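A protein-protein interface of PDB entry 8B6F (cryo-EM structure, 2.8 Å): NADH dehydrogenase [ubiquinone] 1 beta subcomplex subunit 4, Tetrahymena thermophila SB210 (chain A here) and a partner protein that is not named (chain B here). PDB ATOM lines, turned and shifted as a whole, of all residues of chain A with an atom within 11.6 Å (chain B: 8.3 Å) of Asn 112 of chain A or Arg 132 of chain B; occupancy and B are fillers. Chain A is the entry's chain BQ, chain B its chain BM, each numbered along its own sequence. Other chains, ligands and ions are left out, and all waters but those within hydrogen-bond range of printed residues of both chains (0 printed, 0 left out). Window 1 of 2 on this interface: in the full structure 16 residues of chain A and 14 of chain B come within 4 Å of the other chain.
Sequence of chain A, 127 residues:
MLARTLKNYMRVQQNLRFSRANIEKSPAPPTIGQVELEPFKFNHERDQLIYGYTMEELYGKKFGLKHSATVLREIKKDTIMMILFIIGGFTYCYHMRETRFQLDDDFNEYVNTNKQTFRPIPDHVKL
NH2 of Arg 132 of chain B lies close to ND2 of Asn 112 of chain A (3.3 Å).
NE of Arg 132 of chain B lies within hydrogen-bond range of O of Lys 115 of chain A (2.6 Å).
The side-chain hydroxyl of Thr 117 of chain A lies within hydrogen-bond range of the backbone carbonyl oxygen of Asp 133 of chain B (2.8 Å).
The backbone carbonyl oxygen (O) of Phe 134 of chain B sits at hydrogen-bond distance from the side-chain hydroxyl (OG1) of Thr 117 of chain A (2.7 Å).
O of Asn 114 of chain A sits at hydrogen-bond distance from N of Asp 135 of chain B (3.0 Å).
O of Thr 117 of chain A lies close to O of Gly 131 of chain B (3.5 Å).
The side-chain amide oxygen of Asn 120 of chain B lies close to the side-chain amide oxygen of Asn 118 of chain B.
The backbone NH (N) of Asn 118 of chain B lies within hydrogen-bond range of the backbone carbonyl oxygen (O) of Cys 123 of chain B (2.6 Å).
The backbone carbonyl oxygen (O) of Asn 108 of chain A lies within hydrogen-bond range of the side-chain amide nitrogen (ND2) of Asn 112 of chain A (3.1 Å).
O of Asn 112 of chain A is in hydrogen-bond range of NE2 of Gln 116 of chain A.
The side-chain sulfur (SG) of Cys 123 of chain B is disulfide-bonded to the side-chain sulfur (SG) of Cys 130 of chain B (2.0 Å).
Among the printed residues, merely in contact across the chains: Asn 114 of chain A with Phe 134 of chain B (3.8 Å), Lys 115 of chain A with Asp 133 of chain B (3.2 Å), Lys 115 of chain A with Phe 134 of chain B (3.9 Å), Gln 116 of chain A with Asp 133 of chain B (3.6 Å), Gln 116 of chain A with Asp 135 of chain B (3.9 Å), Thr 117 of chain A with Arg 132 of chain B (3.9 Å), Thr 117 of chain A with Asp 135 of chain B (3.2 Å), Phe 118 of chain A with Gly 129 of chain B (3.97 Å), Phe 118 of chain A with Gly 131 of chain B (2.8 Å), Phe 118 of chain A with Arg 132 of chain B (3.4 Å), Arg 119 of chain A with Asp 133 of chain B (3.9 Å) and Ile 121 of chain A with Asn 118 of chain B (3.4 Å).
Asp 104 of chain A touches none of the printed residues of chain B.
Asn 112 of chain A touches just one residue of chain B: Arg 132 (3.1 Å).
Printed residues of chain B within 4 Å of Lys 115 of chain A: Arg 132, Asp 133 and Phe 134.
Printed residues of chain B within 4 Å of Phe 118 of chain A: Gly 129, Gly 131 and Arg 132.
Of the printed residues of chain B, Ile 121 of chain A touches Asn 118 (3.4 Å).
Printed residues of chain A within 4 Å of Asn 118 of chain B: Ile 121.
Phe 121 of chain B touches none of the printed residues of chain A.
Of the printed residues of chain A, Arg 132 of chain B touches Asn 112, Lys 115, Thr 117 and Phe 118.
Phe 134 of chain B touches just these residues of chain A: Asn 114, Lys 115 and Thr 117.
The nearest residue of chain A that does not touch Arg 132 of chain B is Gln 116 of chain A (4.1 Å).
The nearest printed residue of chain B that does not touch Asn 114 of chain A is Asp 133 of chain B (4.3 Å).
Of the 19 printed residues of chain A, 8 touch a printed residue of chain B.
Among the printed residues, 18 pairs touch across the chains.
Among the printed residues, no Asp or Glu carboxylate lies within 4 Å of a Lys or Arg side-chain nitrogen of the other chain.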
ATOM      1  N   LEU A 103      29.737  14.371   9.624  1.00  0.00           N
ATOM      2  CA  LEU A 103      30.736  13.919   8.660  1.00  0.00           C
ATOM      3  C   LEU A 103      30.243  14.107   7.232  1.00  0.00           C
ATOM      4  O   LEU A 103      31.007  14.518   6.352  1.00  0.00           O
ATOM      5  CB  LEU A 103      31.089  12.455   8.916  1.00  0.00           C
ATOM      6  CG  LEU A 103      31.789  12.148  10.239  1.00  0.00           C
ATOM      7  CD1 LEU A 103      31.952  10.652  10.410  1.00  0.00           C
ATOM      8  CD2 LEU A 103      33.139  12.843  10.321  1.00  0.00           C
ATOM      9  N   ASP A 104      28.969  13.798   6.979  1.00  0.00           N
ATOM     10  CA  ASP A 104      28.412  14.004   5.647  1.00  0.00           C
ATOM     11  C   ASP A 104      28.464  15.475   5.254  1.00  0.00           C
ATOM     12  O   ASP A 104      28.809  15.806   4.115  1.00  0.00           O
ATOM     13  CB  ASP A 104      26.973  13.488   5.590  1.00  0.00           C
ATOM     14  CG  ASP A 104      26.897  11.976   5.491  1.00  0.00           C
ATOM     15  OD1 ASP A 104      27.777  11.375   4.843  1.00  0.00           O
ATOM     16  OD2 ASP A 104      25.952  11.389   6.057  1.00  0.00           O
ATOM     17  N   ASP A 105      28.125  16.372   6.183  1.00  0.00           N
ATOM     18  CA  ASP A 105      28.196  17.799   5.885  1.00  0.00           C
ATOM     19  C   ASP A 105      29.617  18.217   5.542  1.00  0.00           C
ATOM     20  O   ASP A 105      29.838  18.967   4.585  1.00  0.00           O
ATOM     21  CB  ASP A 105      27.687  18.615   7.074  1.00  0.00           C
ATOM     22  CG  ASP A 105      26.180  18.604   7.194  1.00  0.00           C
ATOM     23  OD1 ASP A 105      25.501  18.633   6.147  1.00  0.00           O
ATOM     24  OD2 ASP A 105      25.671  18.572   8.334  1.00  0.00           O
ATOM     25  N   ASP A 106      30.594  17.755   6.322  1.00  0.00           N
ATOM     26  CA  ASP A 106      31.981  18.117   6.057  1.00  0.00           C
ATOM     27  C   ASP A 106      32.419  17.644   4.678  1.00  0.00           C
ATOM     28  O   ASP A 106      33.039  18.397   3.918  1.00  0.00           O
ATOM     29  CB  ASP A 106      32.888  17.523   7.134  1.00  0.00           C
ATOM     30  CG  ASP A 106      32.520  17.985   8.527  1.00  0.00           C
ATOM     31  OD1 ASP A 106      31.644  18.865   8.650  1.00  0.00           O
ATOM     32  OD2 ASP A 106      33.103  17.465   9.499  1.00  0.00           O
ATOM     33  N   PHE A 107      32.102  16.395   4.333  1.00  0.00           N
ATOM     34  CA  PHE A 107      32.532  15.863   3.046  1.00  0.00           C
ATOM     35  C   PHE A 107      31.819  16.558   1.895  1.00  0.00           C
ATOM     36  O   PHE A 107      32.412  16.783   0.836  1.00  0.00           O
ATOM     37  CB  PHE A 107      32.302  14.354   2.988  1.00  0.00           C
ATOM     38  CG  PHE A 107      32.980  13.694   1.827  1.00  0.00           C
ATOM     39  CD1 PHE A 107      34.318  13.346   1.903  1.00  0.00           C
ATOM     40  CD2 PHE A 107      32.288  13.431   0.658  1.00  0.00           C
ATOM     41  CE1 PHE A 107      34.951  12.742   0.839  1.00  0.00           C
ATOM     42  CE2 PHE A 107      32.917  12.828  -0.411  1.00  0.00           C
ATOM     43  CZ  PHE A 107      34.250  12.483  -0.321  1.00  0.00           C
ATOM     44  N   ASN A 108      30.546  16.912   2.085  1.00  0.00           N
ATOM     45  CA  ASN A 108      29.834  17.654   1.052  1.00  0.00           C
ATOM     46  C   ASN A 108      30.486  19.007   0.812  1.00  0.00           C
ATOM     47  O   ASN A 108      30.641  19.436  -0.336  1.00  0.00           O
ATOM     48  CB  ASN A 108      28.365  17.826   1.438  1.00  0.00           C
ATOM     49  CG  ASN A 108      27.602  16.519   1.427  1.00  0.00           C
ATOM     50  OD1 ASN A 108      27.964  15.583   0.716  1.00  0.00           O
ATOM     51  ND2 ASN A 108      26.532  16.449   2.211  1.00  0.00           N
ATOM     52  N   GLU A 109      30.868  19.701   1.885  1.00  0.00           N
ATOM     53  CA  GLU A 109      31.585  20.959   1.722  1.00  0.00           C
ATOM     54  C   GLU A 109      32.870  20.748   0.932  1.00  0.00           C
ATOM     55  O   GLU A 109      33.161  21.489  -0.013  1.00  0.00           O
ATOM     56  CB  GLU A 109      31.892  21.564   3.093  1.00  0.00           C
ATOM     57  CG  GLU A 109      30.664  22.023   3.860  1.00  0.00           C
ATOM     58  CD  GLU A 109      29.997  23.227   3.227  1.00  0.00           C
ATOM     59  OE1 GLU A 109      30.584  23.806   2.291  1.00  0.00           O
ATOM     60  OE2 GLU A 109      28.886  23.594   3.664  1.00  0.00           O
ATOM     61  N   TYR A 110      33.658  19.742   1.314  1.00  0.00           N
ATOM     62  CA  TYR A 110      34.918  19.480   0.623  1.00  0.00           C
ATOM     63  C   TYR A 110      34.697  19.229  -0.864  1.00  0.00           C
ATOM     64  O   TYR A 110      35.377  19.817  -1.714  1.00  0.00           O
ATOM     65  CB  TYR A 110      35.627  18.287   1.260  1.00  0.00           C
ATOM     66  CG  TYR A 110      36.531  17.553   0.299  1.00  0.00           C
ATOM     67  CD1 TYR A 110      37.726  18.114  -0.126  1.00  0.00           C
ATOM     68  CD2 TYR A 110      36.187  16.299  -0.183  1.00  0.00           C
ATOM     69  CE1 TYR A 110      38.553  17.447  -1.008  1.00  0.00           C
ATOM     70  CE2 TYR A 110      37.007  15.624  -1.065  1.00  0.00           C
ATOM     71  CZ  TYR A 110      38.188  16.202  -1.472  1.00  0.00           C
ATOM     72  OH  TYR A 110      39.005  15.531  -2.349  1.00  0.00           O
ATOM     73  N   VAL A 111      33.744  18.358  -1.198  1.00  0.00           N
ATOM     74  CA  VAL A 111      33.518  17.994  -2.596  1.00  0.00           C
ATOM     75  C   VAL A 111      33.042  19.202  -3.391  1.00  0.00           C
ATOM     76  O   VAL A 111      33.533  19.478  -4.491  1.00  0.00           O
ATOM     77  CB  VAL A 111      32.519  16.827  -2.691  1.00  0.00           C
ATOM     78  CG1 VAL A 111      32.101  16.584  -4.135  1.00  0.00           C
ATOM     79  CG2 VAL A 111      33.121  15.568  -2.104  1.00  0.00           C
ATOM     80  N   ASN A 112      32.079  19.942  -2.847  1.00  0.00           N
ATOM     81  CA  ASN A 112      31.524  21.083  -3.562  1.00  0.00           C
ATOM     82  C   ASN A 112      32.484  22.262  -3.635  1.00  0.00           C
ATOM     83  O   ASN A 112      32.191  23.223  -4.350  1.00  0.00           O
ATOM     84  CB  ASN A 112      30.221  21.530  -2.896  1.00  0.00           C
ATOM     85  CG  ASN A 112      29.167  20.442  -2.889  1.00  0.00           C
ATOM     86  OD1 ASN A 112      29.195  19.532  -3.716  1.00  0.00           O
ATOM     87  ND2 ASN A 112      28.227  20.533  -1.955  1.00  0.00           N
ATOM     88  N   THR A 113      33.597  22.222  -2.900  1.00  0.00           N
ATOM     89  CA  THR A 113      34.601  23.278  -2.988  1.00  0.00           C
ATOM     90  C   THR A 113      34.830  23.749  -4.419  1.00  0.00           C
ATOM     91  O   THR A 113      34.795  24.950  -4.701  1.00  0.00           O
ATOM     92  CB  THR A 113      35.920  22.792  -2.377  1.00  0.00           C
ATOM     93  OG1 THR A 113      35.750  22.577  -0.970  1.00  0.00           O
ATOM     94  CG2 THR A 113      37.038  23.807  -2.616  1.00  0.00           C
ATOM     95  N   ASN A 114      35.067  22.813  -5.338  1.00  0.00           N
ATOM     96  CA  ASN A 114      35.406  23.157  -6.711  1.00  0.00           C
ATOM     97  C   ASN A 114      34.301  22.861  -7.716  1.00  0.00           C
ATOM     98  O   ASN A 114      34.423  23.270  -8.875  1.00  0.00           O
ATOM     99  CB  ASN A 114      36.682  22.418  -7.138  1.00  0.00           C
ATOM    100  CG  ASN A 114      37.944  23.173  -6.765  1.00  0.00           C
ATOM    101  OD1 ASN A 114      37.976  24.402  -6.791  1.00  0.00           O
ATOM    102  ND2 ASN A 114      38.992  22.437  -6.409  1.00  0.00           N
ATOM    103  N   LYS A 115      33.238  22.162  -7.318  1.00  0.00           N
ATOM    104  CA  LYS A 115      32.129  21.857  -8.220  1.00  0.00           C
ATOM    105  C   LYS A 115      31.018  22.872  -7.970  1.00  0.00           C
ATOM    106  O   LYS A 115      30.002  22.584  -7.337  1.00  0.00           O
ATOM    107  CB  LYS A 115      31.650  20.424  -8.013  1.00  0.00           C
ATOM    108  CG  LYS A 115      32.722  19.377  -8.259  1.00  0.00           C
ATOM    109  CD  LYS A 115      32.195  17.966  -8.055  1.00  0.00           C
ATOM    110  CE  LYS A 115      31.183  17.585  -9.123  1.00  0.00           C
ATOM    111  NZ  LYS A 115      30.737  16.171  -8.984  1.00  0.00           N
ATOM    112  N   GLN A 116      31.219  24.081  -8.492  1.00  0.00           N
ATOM    113  CA  GLN A 116      30.301  25.187  -8.264  1.00  0.00           C
ATOM    114  C   GLN A 116      29.601  25.664  -9.529  1.00  0.00           C
ATOM    115  O   GLN A 116      28.790  26.593  -9.455  1.00  0.00           O
ATOM    116  CB  GLN A 116      31.048  26.364  -7.626  1.00  0.00           C
ATOM    117  CG  GLN A 116      31.609  26.073  -6.244  1.00  0.00           C
ATOM    118  CD  GLN A 116      30.525  25.905  -5.200  1.00  0.00           C
ATOM    119  OE1 GLN A 116      29.340  26.069  -5.486  1.00  0.00           O
ATOM    120  NE2 GLN A 116      30.927  25.578  -3.977  1.00  0.00           N
ATOM    121  N   THR A 117      29.881  25.060 -10.679  1.00  0.00           N
ATOM    122  CA  THR A 117      29.324  25.501 -11.950  1.00  0.00           C
ATOM    123  C   THR A 117      28.075  24.698 -12.283  1.00  0.00           C
ATOM    124  O   THR A 117      28.096  23.464 -12.248  1.00  0.00           O
ATOM    125  CB  THR A 117      30.349  25.363 -13.077  1.00  0.00           C
ATOM    126  OG1 THR A 117      30.966  24.070 -13.017  1.00  0.00           O
ATOM    127  CG2 THR A 117      31.405  26.448 -12.965  1.00  0.00           C
ATOM    128  N   PHE A 118      26.995  25.403 -12.605  1.00  0.00           N
ATOM    129  CA  PHE A 118      25.744  24.796 -13.037  1.00  0.00           C
ATOM    130  C   PHE A 118      25.462  25.259 -14.458  1.00  0.00           C
ATOM    131  O   PHE A 118      25.394  26.465 -14.718  1.00  0.00           O
ATOM    132  CB  PHE A 118      24.594  25.179 -12.103  1.00  0.00           C
ATOM    133  CG  PHE A 118      24.843  24.836 -10.663  1.00  0.00           C
ATOM    134  CD1 PHE A 118      25.614  25.665  -9.865  1.00  0.00           C
ATOM    135  CD2 PHE A 118      24.300  23.691 -10.106  1.00  0.00           C
ATOM    136  CE1 PHE A 118      25.845  25.352  -8.540  1.00  0.00           C
ATOM    137  CE2 PHE A 118      24.526  23.373  -8.784  1.00  0.00           C
ATOM    138  CZ  PHE A 118      25.299  24.205  -7.999  1.00  0.00           C
ATOM    139  N   ARG A 119      25.302  24.304 -15.374  1.00  0.00           N
ATOM    140  CA  ARG A 119      25.050  24.619 -16.771  1.00  0.00           C
ATOM    141  C   ARG A 119      23.562  24.501 -17.060  1.00  0.00           C
ATOM    142  O   ARG A 119      23.003  23.405 -16.904  1.00  0.00           O
ATOM    143  CB  ARG A 119      25.837  23.688 -17.680  1.00  0.00           C
ATOM    144  CG  ARG A 119      27.336  23.948 -17.668  1.00  0.00           C
ATOM    145  CD  ARG A 119      28.046  23.168 -18.760  1.00  0.00           C
ATOM    146  NE  ARG A 119      27.496  23.456 -20.080  1.00  0.00           N
ATOM    147  CZ  ARG A 119      27.753  24.552 -20.779  1.00  0.00           C
ATOM    148  NH1 ARG A 119      28.547  25.502 -20.310  1.00  0.00           N
ATOM    149  NH2 ARG A 119      27.198  24.703 -21.977  1.00  0.00           N
ATOM    150  N   PRO A 120      22.884  25.570 -17.478  1.00  0.00           N
ATOM    151  CA  PRO A 120      21.447  25.459 -17.753  1.00  0.00           C
ATOM    152  C   PRO A 120      21.169  24.541 -18.932  1.00  0.00           C
ATOM    153  O   PRO A 120      21.982  24.397 -19.846  1.00  0.00           O
ATOM    154  CB  PRO A 120      21.034  26.901 -18.063  1.00  0.00           C
ATOM    155  CG  PRO A 120      22.274  27.546 -18.557  1.00  0.00           C
ATOM    156  CD  PRO A 120      23.399  26.913 -17.795  1.00  0.00           C
ATOM    157  N   ILE A 121      20.000  23.915 -18.897  1.00  0.00           N
ATOM    158  CA  ILE A 121      19.604  23.016 -19.986  1.00  0.00           C
ATOM    159  C   ILE A 121      19.399  23.833 -21.256  1.00  0.00           C
ATOM    160  O   ILE A 121      18.895  24.968 -21.180  1.00  0.00           O
ATOM    161  CB  ILE A 121      18.333  22.250 -19.608  1.00  0.00           C
ATOM    162  CG1 ILE A 121      18.556  21.463 -18.312  1.00  0.00           C
ATOM    163  CG2 ILE A 121      17.927  21.309 -20.737  1.00  0.00           C
ATOM    164  CD1 ILE A 121      17.329  20.730 -17.804  1.00  0.00           C
ATOM    165  N   ASN B 118      17.478  16.942 -16.873  1.00  0.00           N
ATOM    166  CA  ASN B 118      18.861  17.091 -17.311  1.00  0.00           C
ATOM    167  C   ASN B 118      19.357  15.734 -17.793  1.00  0.00           C
ATOM    168  O   ASN B 118      19.602  14.832 -16.987  1.00  0.00           O
ATOM    169  CB  ASN B 118      19.720  17.624 -16.168  1.00  0.00           C
ATOM    170  CG  ASN B 118      20.889  18.447 -16.654  1.00  0.00           C
ATOM    171  OD1 ASN B 118      21.869  17.912 -17.165  1.00  0.00           O
ATOM    172  ND2 ASN B 118      20.798  19.760 -16.484  1.00  0.00           N
ATOM    173  N   ASN B 120      22.194  14.539 -19.375  1.00  0.00           N
ATOM    174  CA  ASN B 120      23.540  14.057 -19.092  1.00  0.00           C
ATOM    175  C   ASN B 120      23.862  14.027 -17.606  1.00  0.00           C
ATOM    176  O   ASN B 120      24.909  13.489 -17.231  1.00  0.00           O
ATOM    177  CB  ASN B 120      24.574  14.909 -19.831  1.00  0.00           C
ATOM    178  CG  ASN B 120      24.397  16.388 -19.582  1.00  0.00           C
ATOM    179  OD1 ASN B 120      23.731  16.794 -18.633  1.00  0.00           O
ATOM    180  ND2 ASN B 120      24.995  17.206 -20.439  1.00  0.00           N
ATOM    181  N   PHE B 121      23.002  14.588 -16.754  1.00  0.00           N
ATOM    182  CA  PHE B 121      23.170  14.495 -15.313  1.00  0.00           C
ATOM    183  C   PHE B 121      22.042  13.748 -14.620  1.00  0.00           C
ATOM    184  O   PHE B 121      22.133  13.517 -13.409  1.00  0.00           O
ATOM    185  CB  PHE B 121      23.302  15.896 -14.695  1.00  0.00           C
ATOM    186  CG  PHE B 121      24.623  16.547 -14.974  1.00  0.00           C
ATOM    187  CD1 PHE B 121      25.764  16.131 -14.311  1.00  0.00           C
ATOM    188  CD2 PHE B 121      24.726  17.566 -15.904  1.00  0.00           C
ATOM    189  CE1 PHE B 121      26.984  16.723 -14.567  1.00  0.00           C
ATOM    190  CE2 PHE B 121      25.943  18.163 -16.165  1.00  0.00           C
ATOM    191  CZ  PHE B 121      27.075  17.740 -15.494  1.00  0.00           C
ATOM    192  N   CYS B 123      18.692  14.249 -13.738  1.00  0.00           N
ATOM    193  CA  CYS B 123      17.964  14.891 -12.651  1.00  0.00           C
ATOM    194  C   CYS B 123      17.130  16.024 -13.224  1.00  0.00           C
ATOM    195  O   CYS B 123      17.380  16.504 -14.333  1.00  0.00           O
ATOM    196  CB  CYS B 123      18.910  15.416 -11.568  1.00  0.00           C
ATOM    197  SG  CYS B 123      20.327  16.337 -12.197  1.00  0.00           S
ATOM    198  N   PRO B 128      17.719  19.753  -5.886  1.00  0.00           N
ATOM    199  CA  PRO B 128      18.915  20.471  -5.423  1.00  0.00           C
ATOM    200  C   PRO B 128      20.178  19.953  -6.095  1.00  0.00           C
ATOM    201  O   PRO B 128      20.408  18.745  -6.179  1.00  0.00           O
ATOM    202  CB  PRO B 128      18.927  20.203  -3.912  1.00  0.00           C
ATOM    203  CG  PRO B 128      17.531  19.854  -3.570  1.00  0.00           C
ATOM    204  CD  PRO B 128      16.979  19.145  -4.765  1.00  0.00           C
ATOM    205  N   GLY B 129      21.000  20.883  -6.570  1.00  0.00           N
ATOM    206  CA  GLY B 129      22.285  20.526  -7.150  1.00  0.00           C
ATOM    207  C   GLY B 129      22.191  19.529  -8.285  1.00  0.00           C
ATOM    208  O   GLY B 129      22.993  18.590  -8.349  1.00  0.00           O
ATOM    209  N   CYS B 130      21.227  19.712  -9.188  1.00  0.00           N
ATOM    210  CA  CYS B 130      21.047  18.758 -10.276  1.00  0.00           C
ATOM    211  C   CYS B 130      22.284  18.699 -11.163  1.00  0.00           C
ATOM    212  O   CYS B 130      22.956  17.664 -11.249  1.00  0.00           O
ATOM    213  CB  CYS B 130      19.805  19.127 -11.092  1.00  0.00           C
ATOM    214  SG  CYS B 130      19.608  18.189 -12.628  1.00  0.00           S
ATOM    215  N   GLY B 131      22.606  19.805 -11.827  1.00  0.00           N
ATOM    216  CA  GLY B 131      23.783  19.848 -12.671  1.00  0.00           C
ATOM    217  C   GLY B 131      24.983  20.417 -11.949  1.00  0.00           C
ATOM    218  O   GLY B 131      25.146  21.638 -11.878  1.00  0.00           O
ATOM    219  N   ARG B 132      25.839  19.548 -11.420  1.00  0.00           N
ATOM    220  CA  ARG B 132      27.016  19.953 -10.661  1.00  0.00           C
ATOM    221  C   ARG B 132      28.248  19.604 -11.483  1.00  0.00           C
ATOM    222  O   ARG B 132      28.582  18.426 -11.642  1.00  0.00           O
ATOM    223  CB  ARG B 132      27.045  19.266  -9.297  1.00  0.00           C
ATOM    224  CG  ARG B 132      27.789  20.041  -8.219  1.00  0.00           C
ATOM    225  CD  ARG B 132      27.127  21.380  -7.952  1.00  0.00           C
ATOM    226  NE  ARG B 132      27.594  22.003  -6.720  1.00  0.00           N
ATOM    227  CZ  ARG B 132      27.045  21.819  -5.528  1.00  0.00           C
ATOM    228  NH1 ARG B 132      26.019  21.000  -5.357  1.00  0.00           N
ATOM    229  NH2 ARG B 132      27.531  22.477  -4.481  1.00  0.00           N
ATOM    230  N   ASP B 133      28.921  20.628 -11.998  1.00  0.00           N
ATOM    231  CA  ASP B 133      30.056  20.456 -12.887  1.00  0.00           C
ATOM    232  C   ASP B 133      31.311  21.025 -12.241  1.00  0.00           C
ATOM    233  O   ASP B 133      31.247  21.838 -11.316  1.00  0.00           O
ATOM    234  CB  ASP B 133      29.801  21.138 -14.236  1.00  0.00           C
ATOM    235  CG  ASP B 133      30.261  20.300 -15.408  1.00  0.00           C
ATOM    236  OD1 ASP B 133      31.259  19.564 -15.260  1.00  0.00           O
ATOM    237  OD2 ASP B 133      29.622  20.374 -16.477  1.00  0.00           O
ATOM    238  N   PHE B 134      32.461  20.586 -12.744  1.00  0.00           N
ATOM    239  CA  PHE B 134      33.734  21.005 -12.186  1.00  0.00           C
ATOM    240  C   PHE B 134      34.044  22.451 -12.564  1.00  0.00           C
ATOM    241  O   PHE B 134      33.433  23.036 -13.463  1.00  0.00           O
ATOM    242  CB  PHE B 134      34.855  20.085 -12.664  1.00  0.00           C
ATOM    243  CG  PHE B 134      34.733  18.679 -12.164  1.00  0.00           C
ATOM    244  CD1 PHE B 134      34.017  17.736 -12.878  1.00  0.00           C
ATOM    245  CD2 PHE B 134      35.327  18.303 -10.972  1.00  0.00           C
ATOM    246  CE1 PHE B 134      33.900  16.441 -12.415  1.00  0.00           C
ATOM    247  CE2 PHE B 134      35.215  17.011 -10.504  1.00  0.00           C
ATOM    248  CZ  PHE B 134      34.499  16.078 -11.226  1.00  0.00           C
ATOM    249  N   ASP B 135      35.011  23.026 -11.856  1.00  0.00           N
ATOM    250  CA  ASP B 135      35.408  24.413 -12.063  1.00  0.00           C
ATOM    251  C   ASP B 135      34.224  25.348 -11.870  1.00  0.00           C
ATOM    252  O   ASP B 135      33.939  25.781 -10.753  1.00  0.00           O
ATOM    253  CB  ASP B 135      36.005  24.606 -13.459  1.00  0.00           C
ATOM    254  CG  ASP B 135      37.260  23.783 -13.675  1.00  0.00           C
ATOM    255  OD1 ASP B 135      37.981  23.526 -12.688  1.00  0.00           O
ATOM    256  OD2 ASP B 135      37.525  23.393 -14.830  1.00  0.00           O
